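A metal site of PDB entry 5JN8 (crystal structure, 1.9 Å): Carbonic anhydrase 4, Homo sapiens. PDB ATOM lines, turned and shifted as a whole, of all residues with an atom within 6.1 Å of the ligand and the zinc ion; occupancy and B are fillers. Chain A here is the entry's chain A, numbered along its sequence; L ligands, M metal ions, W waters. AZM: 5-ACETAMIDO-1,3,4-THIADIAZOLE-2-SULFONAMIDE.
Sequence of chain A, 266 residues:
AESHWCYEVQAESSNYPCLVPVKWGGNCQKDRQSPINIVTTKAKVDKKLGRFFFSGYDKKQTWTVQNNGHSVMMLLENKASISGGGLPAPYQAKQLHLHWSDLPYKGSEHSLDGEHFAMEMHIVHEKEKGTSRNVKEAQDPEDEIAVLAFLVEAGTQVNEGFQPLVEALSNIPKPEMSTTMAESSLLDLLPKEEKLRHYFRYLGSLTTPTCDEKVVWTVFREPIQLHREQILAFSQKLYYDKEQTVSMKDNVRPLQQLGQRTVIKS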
ATOM      1  N   MET A  73     -22.418 -22.681 -10.376  1.00  0.00           N
ATOM      2  CA  MET A  73     -21.180 -22.209  -9.796  1.00  0.00           C
ATOM      3  C   MET A  73     -20.427 -23.327  -9.055  1.00  0.00           C
ATOM      4  O   MET A  73     -20.976 -23.958  -8.146  1.00  0.00           O
ATOM      5  CB  MET A  73     -21.518 -21.068  -8.830  1.00  0.00           C
ATOM      6  CG  MET A  73     -20.357 -20.329  -8.299  1.00  0.00           C
ATOM      7  SD  MET A  73     -20.844 -19.021  -7.131  1.00  0.00           S
ATOM      8  CE  MET A  73     -21.941 -19.897  -6.022  1.00  0.00           C
ATOM      9  N   GLN A  95     -14.435 -18.977  -7.451  1.00  0.00           N
ATOM     10  CA  GLN A  95     -15.549 -19.736  -8.042  1.00  0.00           C
ATOM     11  C   GLN A  95     -15.448 -19.766  -9.540  1.00  0.00           C
ATOM     12  O   GLN A  95     -14.764 -18.943 -10.117  1.00  0.00           O
ATOM     13  CB  GLN A  95     -16.889 -19.161  -7.595  1.00  0.00           C
ATOM     14  CG  GLN A  95     -16.974 -17.644  -7.682  1.00  0.00           C
ATOM     15  CD  GLN A  95     -17.997 -17.163  -8.676  1.00  0.00           C
ATOM     16  OE1 GLN A  95     -18.336 -17.870  -9.629  1.00  0.00           O
ATOM     17  NE2 GLN A  95     -18.519 -15.967  -8.452  1.00  0.00           N
ATOM     18  N   HIS A  97     -18.163 -20.119 -12.884  1.00  0.00           N
ATOM     19  CA  HIS A  97     -19.564 -20.184 -13.290  1.00  0.00           C
ATOM     20  C   HIS A  97     -19.660 -19.931 -14.796  1.00  0.00           C
ATOM     21  O   HIS A  97     -18.646 -19.677 -15.469  1.00  0.00           O
ATOM     22  CB  HIS A  97     -20.412 -19.179 -12.495  1.00  0.00           C
ATOM     23  CG  HIS A  97     -20.057 -17.761 -12.787  1.00  0.00           C
ATOM     24  ND1 HIS A  97     -19.246 -16.996 -11.971  1.00  0.00           N
ATOM     25  CD2 HIS A  97     -20.342 -16.976 -13.862  1.00  0.00           C
ATOM     26  CE1 HIS A  97     -19.086 -15.808 -12.504  1.00  0.00           C
ATOM     27  NE2 HIS A  97     -19.739 -15.765 -13.646  1.00  0.00           N
ATOM     28  N   LEU A  98     -20.883 -20.022 -15.318  1.00  0.00           N
ATOM     29  CA  LEU A  98     -21.113 -19.935 -16.771  1.00  0.00           C
ATOM     30  C   LEU A  98     -22.348 -19.093 -17.116  1.00  0.00           C
ATOM     31  O   LEU A  98     -23.240 -18.897 -16.287  1.00  0.00           O
ATOM     32  CB  LEU A  98     -21.250 -21.351 -17.392  1.00  0.00           C
ATOM     33  CG  LEU A  98     -20.053 -22.301 -17.328  1.00  0.00           C
ATOM     34  CD1 LEU A  98     -20.149 -23.268 -16.162  1.00  0.00           C
ATOM     35  CD2 LEU A  98     -19.898 -23.097 -18.627  1.00  0.00           C
ATOM     36  N   HIS A  99     -22.361 -18.604 -18.349  1.00  0.00           N
ATOM     37  CA  HIS A  99     -23.484 -17.917 -18.941  1.00  0.00           C
ATOM     38  C   HIS A  99     -23.734 -18.640 -20.264  1.00  0.00           C
ATOM     39  O   HIS A  99     -22.783 -19.080 -20.905  1.00  0.00           O
ATOM     40  CB  HIS A  99     -23.121 -16.455 -19.202  1.00  0.00           C
ATOM     41  CG  HIS A  99     -22.648 -15.722 -17.983  1.00  0.00           C
ATOM     42  ND1 HIS A  99     -23.469 -14.924 -17.217  1.00  0.00           N
ATOM     43  CD2 HIS A  99     -21.432 -15.685 -17.373  1.00  0.00           C
ATOM     44  CE1 HIS A  99     -22.786 -14.394 -16.223  1.00  0.00           C
ATOM     45  NE2 HIS A  99     -21.548 -14.842 -16.292  1.00  0.00           N
ATOM     46  N   GLU A 109     -21.166 -13.563 -22.982  1.00  0.00           N
ATOM     47  CA  GLU A 109     -21.347 -12.197 -22.553  1.00  0.00           C
ATOM     48  C   GLU A 109     -20.537 -11.254 -23.443  1.00  0.00           C
ATOM     49  O   GLU A 109     -21.096 -10.347 -24.079  1.00  0.00           O
ATOM     50  CB  GLU A 109     -20.998 -12.051 -21.062  1.00  0.00           C
ATOM     51  CG  GLU A 109     -22.007 -12.789 -20.171  1.00  0.00           C
ATOM     52  CD  GLU A 109     -22.195 -12.137 -18.819  1.00  0.00           C
ATOM     53  OE1 GLU A 109     -21.211 -12.041 -18.067  1.00  0.00           O
ATOM     54  OE2 GLU A 109     -23.325 -11.714 -18.503  1.00  0.00           O
ATOM     55  N   GLU A 120     -20.220 -18.708 -22.150  1.00  0.00           N
ATOM     56  CA  GLU A 120     -18.989 -18.134 -21.656  1.00  0.00           C
ATOM     57  C   GLU A 120     -18.774 -18.562 -20.212  1.00  0.00           C
ATOM     58  O   GLU A 120     -19.655 -18.406 -19.364  1.00  0.00           O
ATOM     59  CB  GLU A 120     -19.027 -16.613 -21.778  1.00  0.00           C
ATOM     60  CG  GLU A 120     -17.746 -15.905 -21.398  1.00  0.00           C
ATOM     61  CD  GLU A 120     -17.806 -14.435 -21.743  1.00  0.00           C
ATOM     62  OE1 GLU A 120     -18.480 -14.108 -22.746  1.00  0.00           O
ATOM     63  OE2 GLU A 120     -17.221 -13.605 -21.021  1.00  0.00           O
ATOM     64  N   HIS A 122     -16.611 -18.201 -16.712  1.00  0.00           N
ATOM     65  CA  HIS A 122     -15.884 -17.189 -15.950  1.00  0.00           C
ATOM     66  C   HIS A 122     -15.245 -17.839 -14.712  1.00  0.00           C
ATOM     67  O   HIS A 122     -15.955 -18.423 -13.906  1.00  0.00           O
ATOM     68  CB  HIS A 122     -16.832 -16.074 -15.519  1.00  0.00           C
ATOM     69  CG  HIS A 122     -17.284 -15.188 -16.648  1.00  0.00           C
ATOM     70  ND1 HIS A 122     -18.423 -14.415 -16.571  1.00  0.00           N
ATOM     71  CD2 HIS A 122     -16.746 -14.947 -17.865  1.00  0.00           C
ATOM     72  CE1 HIS A 122     -18.562 -13.722 -17.686  1.00  0.00           C
ATOM     73  NE2 HIS A 122     -17.557 -14.028 -18.483  1.00  0.00           N
ATOM     74  N   VAL A 124     -13.359 -16.743 -11.430  1.00  0.00           N
ATOM     75  CA  VAL A 124     -13.281 -15.510 -10.663  1.00  0.00           C
ATOM     76  C   VAL A 124     -12.185 -15.676  -9.597  1.00  0.00           C
ATOM     77  O   VAL A 124     -12.241 -16.604  -8.789  1.00  0.00           O
ATOM     78  CB  VAL A 124     -14.646 -15.178 -10.009  1.00  0.00           C
ATOM     79  CG1 VAL A 124     -14.610 -13.856  -9.279  1.00  0.00           C
ATOM     80  CG2 VAL A 124     -15.786 -15.209 -11.055  1.00  0.00           C
ATOM     81  N   ILE A 145     -10.403  -7.998  -8.577  1.00  0.00           N
ATOM     82  CA  ILE A 145     -10.889  -9.278  -9.082  1.00  0.00           C
ATOM     83  C   ILE A 145     -10.307  -9.538 -10.470  1.00  0.00           C
ATOM     84  O   ILE A 145     -10.317  -8.650 -11.331  1.00  0.00           O
ATOM     85  CB  ILE A 145     -12.450  -9.313  -9.124  1.00  0.00           C
ATOM     86  CG1 ILE A 145     -13.000  -9.293  -7.691  1.00  0.00           C
ATOM     87  CG2 ILE A 145     -12.976 -10.523  -9.919  1.00  0.00           C
ATOM     88  CD1 ILE A 145     -14.457  -8.956  -7.585  1.00  0.00           C
ATOM     89  N   VAL A 147     -11.059 -11.969 -13.549  1.00  0.00           N
ATOM     90  CA  VAL A 147     -11.948 -12.976 -14.136  1.00  0.00           C
ATOM     91  C   VAL A 147     -11.303 -13.481 -15.413  1.00  0.00           C
ATOM     92  O   VAL A 147     -10.856 -12.683 -16.253  1.00  0.00           O
ATOM     93  CB  VAL A 147     -13.379 -12.439 -14.483  1.00  0.00           C
ATOM     94  CG1 VAL A 147     -14.202 -13.551 -15.124  1.00  0.00           C
ATOM     95  CG2 VAL A 147     -14.121 -11.916 -13.233  1.00  0.00           C
ATOM     96  N   SER A 205     -16.050  -4.367 -15.148  1.00  0.00           N
ATOM     97  CA  SER A 205     -16.911  -4.607 -13.986  1.00  0.00           C
ATOM     98  C   SER A 205     -17.320  -6.059 -13.906  1.00  0.00           C
ATOM     99  O   SER A 205     -17.144  -6.830 -14.844  1.00  0.00           O
ATOM    100  CB  SER A 205     -18.154  -3.718 -14.055  1.00  0.00           C
ATOM    101  OG  SER A 205     -19.055  -4.129 -15.066  1.00  0.00           O
ATOM    102  N   LEU A 206     -17.867  -6.431 -12.754  1.00  0.00           N
ATOM    103  CA  LEU A 206     -18.647  -7.652 -12.641  1.00  0.00           C
ATOM    104  C   LEU A 206     -19.897  -7.468 -13.506  1.00  0.00           C
ATOM    105  O   LEU A 206     -20.352  -6.334 -13.743  1.00  0.00           O
ATOM    106  CB  LEU A 206     -19.008  -7.910 -11.169  1.00  0.00           C
ATOM    107  CG  LEU A 206     -17.777  -8.100 -10.258  1.00  0.00           C
ATOM    108  CD1 LEU A 206     -18.012  -7.805  -8.778  1.00  0.00           C
ATOM    109  CD2 LEU A 206     -17.218  -9.510 -10.453  1.00  0.00           C
ATOM    110  N   THR A 207     -20.455  -8.571 -14.016  1.00  0.00           N
ATOM    111  CA  THR A 207     -21.574  -8.448 -14.934  1.00  0.00           C
ATOM    112  C   THR A 207     -22.923  -8.768 -14.298  1.00  0.00           C
ATOM    113  O   THR A 207     -23.901  -8.967 -14.996  1.00  0.00           O
ATOM    114  CB  THR A 207     -21.378  -9.309 -16.203  1.00  0.00           C
ATOM    115  OG1 THR A 207     -21.398 -10.699 -15.858  1.00  0.00           O
ATOM    116  CG2 THR A 207     -20.039  -8.958 -16.904  1.00  0.00           C
ATOM    117  N   THR A 208     -22.955  -8.823 -12.969  1.00  0.00           N
ATOM    118  CA  THR A 208     -24.221  -8.869 -12.239  1.00  0.00           C
ATOM    119  C   THR A 208     -24.186  -7.819 -11.144  1.00  0.00           C
ATOM    120  O   THR A 208     -23.109  -7.438 -10.675  1.00  0.00           O
ATOM    121  CB  THR A 208     -24.546 -10.276 -11.662  1.00  0.00           C
ATOM    122  OG1 THR A 208     -23.522 -10.683 -10.745  1.00  0.00           O
ATOM    123  CG2 THR A 208     -24.649 -11.311 -12.771  1.00  0.00           C
ATOM    124  N   PRO A 209     -25.370  -7.315 -10.741  1.00  0.00           N
ATOM    125  CA  PRO A 209     -25.416  -6.310  -9.664  1.00  0.00           C
ATOM    126  C   PRO A 209     -24.608  -6.775  -8.430  1.00  0.00           C
ATOM    127  O   PRO A 209     -24.694  -7.930  -8.068  1.00  0.00           O
ATOM    128  CB  PRO A 209     -26.921  -6.203  -9.370  1.00  0.00           C
ATOM    129  CG  PRO A 209     -27.558  -6.518 -10.696  1.00  0.00           C
ATOM    130  CD  PRO A 209     -26.718  -7.617 -11.256  1.00  0.00           C
ATOM    131  N   VAL A 215     -12.763  -5.221 -11.759  1.00  0.00           N
ATOM    132  CA  VAL A 215     -12.332  -6.403 -12.486  1.00  0.00           C
ATOM    133  C   VAL A 215     -11.294  -6.119 -13.581  1.00  0.00           C
ATOM    134  O   VAL A 215     -11.506  -5.302 -14.502  1.00  0.00           O
ATOM    135  CB  VAL A 215     -13.547  -7.156 -13.139  1.00  0.00           C
ATOM    136  CG1 VAL A 215     -13.087  -8.412 -13.908  1.00  0.00           C
ATOM    137  CG2 VAL A 215     -14.580  -7.517 -12.086  1.00  0.00           C
ATOM    138  N   TRP A 217     -10.138  -7.950 -16.638  1.00  0.00           N
ATOM    139  CA  TRP A 217     -10.676  -8.983 -17.511  1.00  0.00           C
ATOM    140  C   TRP A 217      -9.636  -9.612 -18.403  1.00  0.00           C
ATOM    141  O   TRP A 217      -8.760  -8.926 -18.943  1.00  0.00           O
ATOM    142  CB  TRP A 217     -11.781  -8.417 -18.395  1.00  0.00           C
ATOM    143  CG  TRP A 217     -13.091  -8.353 -17.701  1.00  0.00           C
ATOM    144  CD1 TRP A 217     -13.642  -7.253 -17.089  1.00  0.00           C
ATOM    145  CD2 TRP A 217     -14.029  -9.417 -17.533  1.00  0.00           C
ATOM    146  NE1 TRP A 217     -14.856  -7.579 -16.550  1.00  0.00           N
ATOM    147  CE2 TRP A 217     -15.122  -8.889 -16.806  1.00  0.00           C
ATOM    148  CE3 TRP A 217     -14.043 -10.760 -17.930  1.00  0.00           C
ATOM    149  CZ2 TRP A 217     -16.246  -9.665 -16.479  1.00  0.00           C
ATOM    150  CZ3 TRP A 217     -15.150 -11.544 -17.596  1.00  0.00           C
ATOM    151  CH2 TRP A 217     -16.234 -10.988 -16.862  1.00  0.00           C
HETATM  152  C1  AZM L   1     -19.488 -11.920 -11.742  1.00  0.00           C
HETATM  153  C2  AZM L   1     -20.013 -12.067  -9.439  1.00  0.00           C
HETATM  154  C3  AZM L   1     -19.402 -13.015  -7.307  1.00  0.00           C
HETATM  155  C4  AZM L   1     -20.288 -13.660  -6.265  1.00  0.00           C
HETATM  156  N1  AZM L   1     -20.115 -12.629 -14.152  1.00  0.00           N
HETATM  157  N2  AZM L   1     -20.886 -11.256 -10.108  1.00  0.00           N
HETATM  158  N3  AZM L   1     -20.580 -11.167 -11.528  1.00  0.00           N
HETATM  159  N4  AZM L   1     -19.960 -12.033  -8.020  1.00  0.00           N
HETATM  160  O1  AZM L   1     -18.512 -10.758 -13.884  1.00  0.00           O
HETATM  161  O2  AZM L   1     -17.753 -13.031 -13.375  1.00  0.00           O
HETATM  162  O3  AZM L   1     -18.230 -13.390  -7.490  1.00  0.00           O
HETATM  163  S1  AZM L   1     -18.840 -12.059 -13.336  1.00  0.00           S
HETATM  164  S2  AZM L   1     -18.856 -12.715 -10.363  1.00  0.00           S
HETATM  165 ZN    ZN M   1     -19.920 -14.321 -15.078  1.00  0.00          ZN
HETATM  166  O   HOH W   1     -21.564  -8.582  -8.580  1.00  0.00           O
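The backbone NH of Thr 207 is in hydrogen-bond range of an oxygen (O1) of the ligand.
The side-chain hydroxyl of Thr 207 is in hydrogen-bond range of an oxygen (O1) of the ligand (3.5 Å).
OG1 of Thr 208 lies within hydrogen-bond range of N2 of the ligand (2.8 Å).
O3 of the ligand lies within hydrogen-bond range of NE2 of Gln 95, at 2.8 Å.
A ring nitrogen (ND1) of His 97 sits at hydrogen-bond distance from the side-chain amide oxygen (OE1) of Gln 95 (2.7 Å).
The side-chain hydroxyl (OG1) of Thr 207 is in hydrogen-bond range of the side-chain carboxylate (OE1) of Glu 109 (2.6 Å).
The side-chain carboxylate (OE2) of Glu 109 sits close to a ring nitrogen (ND1) of His 99 (3.5 Å).
N of Val 124 lies within hydrogen-bond range of O of Gln 95, at 2.9 Å.
OE1 of Glu 120 sits at hydrogen-bond distance from N of Glu 109 (2.8 Å).
The backbone carbonyl oxygen (O) of Ser 205 is in hydrogen-bond range of the indole nitrogen (NE1) of Trp 217, 3.0 Å away.
The backbone carbonyl oxygen of His 99 lies within hydrogen-bond range of the backbone NH of Glu 120 (2.9 Å).
A ring nitrogen (NE2) of His 122 lies within hydrogen-bond range of the side-chain carboxylate (OE2) of Glu 120, 2.6 Å away.
CG2 of Val 124 touches O2 of the ligand (3.7 Å).
Val 147 touches the ligand (CG2 to O2, 3.8 Å).
CA of Leu 206 touches O1 of the ligand (3.3 Å).
Trp 217 touches the ligand (CZ2 to O1, 3.6 Å).
Hydrophobic or aromatic side chains within 4 Å of the ligand: His 97, His 99, His 122, Val 124, Val 147, Leu 206 and Trp 217.
Of the 18 residues printed, 10 come within 4 Å of the ligand.
The nearest printed residue that does not touch the ligand is Glu 109 (4.1 Å).
OE1 of Glu 109 touches the zinc ion, 3.97 Å away.
Thr 207 touches the zinc ion.
The nearest printed residue that does not touch the zinc ion is Trp 217 (5.3 Å).
N1 of the ligand binds the zinc ion.
NE2 of His 97 is bound to the zinc ion (2.0 Å).
NE2 of His 99 is bound to the zinc ion (2.1 Å).
ND1 of His 122 is bound to the zinc ion.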
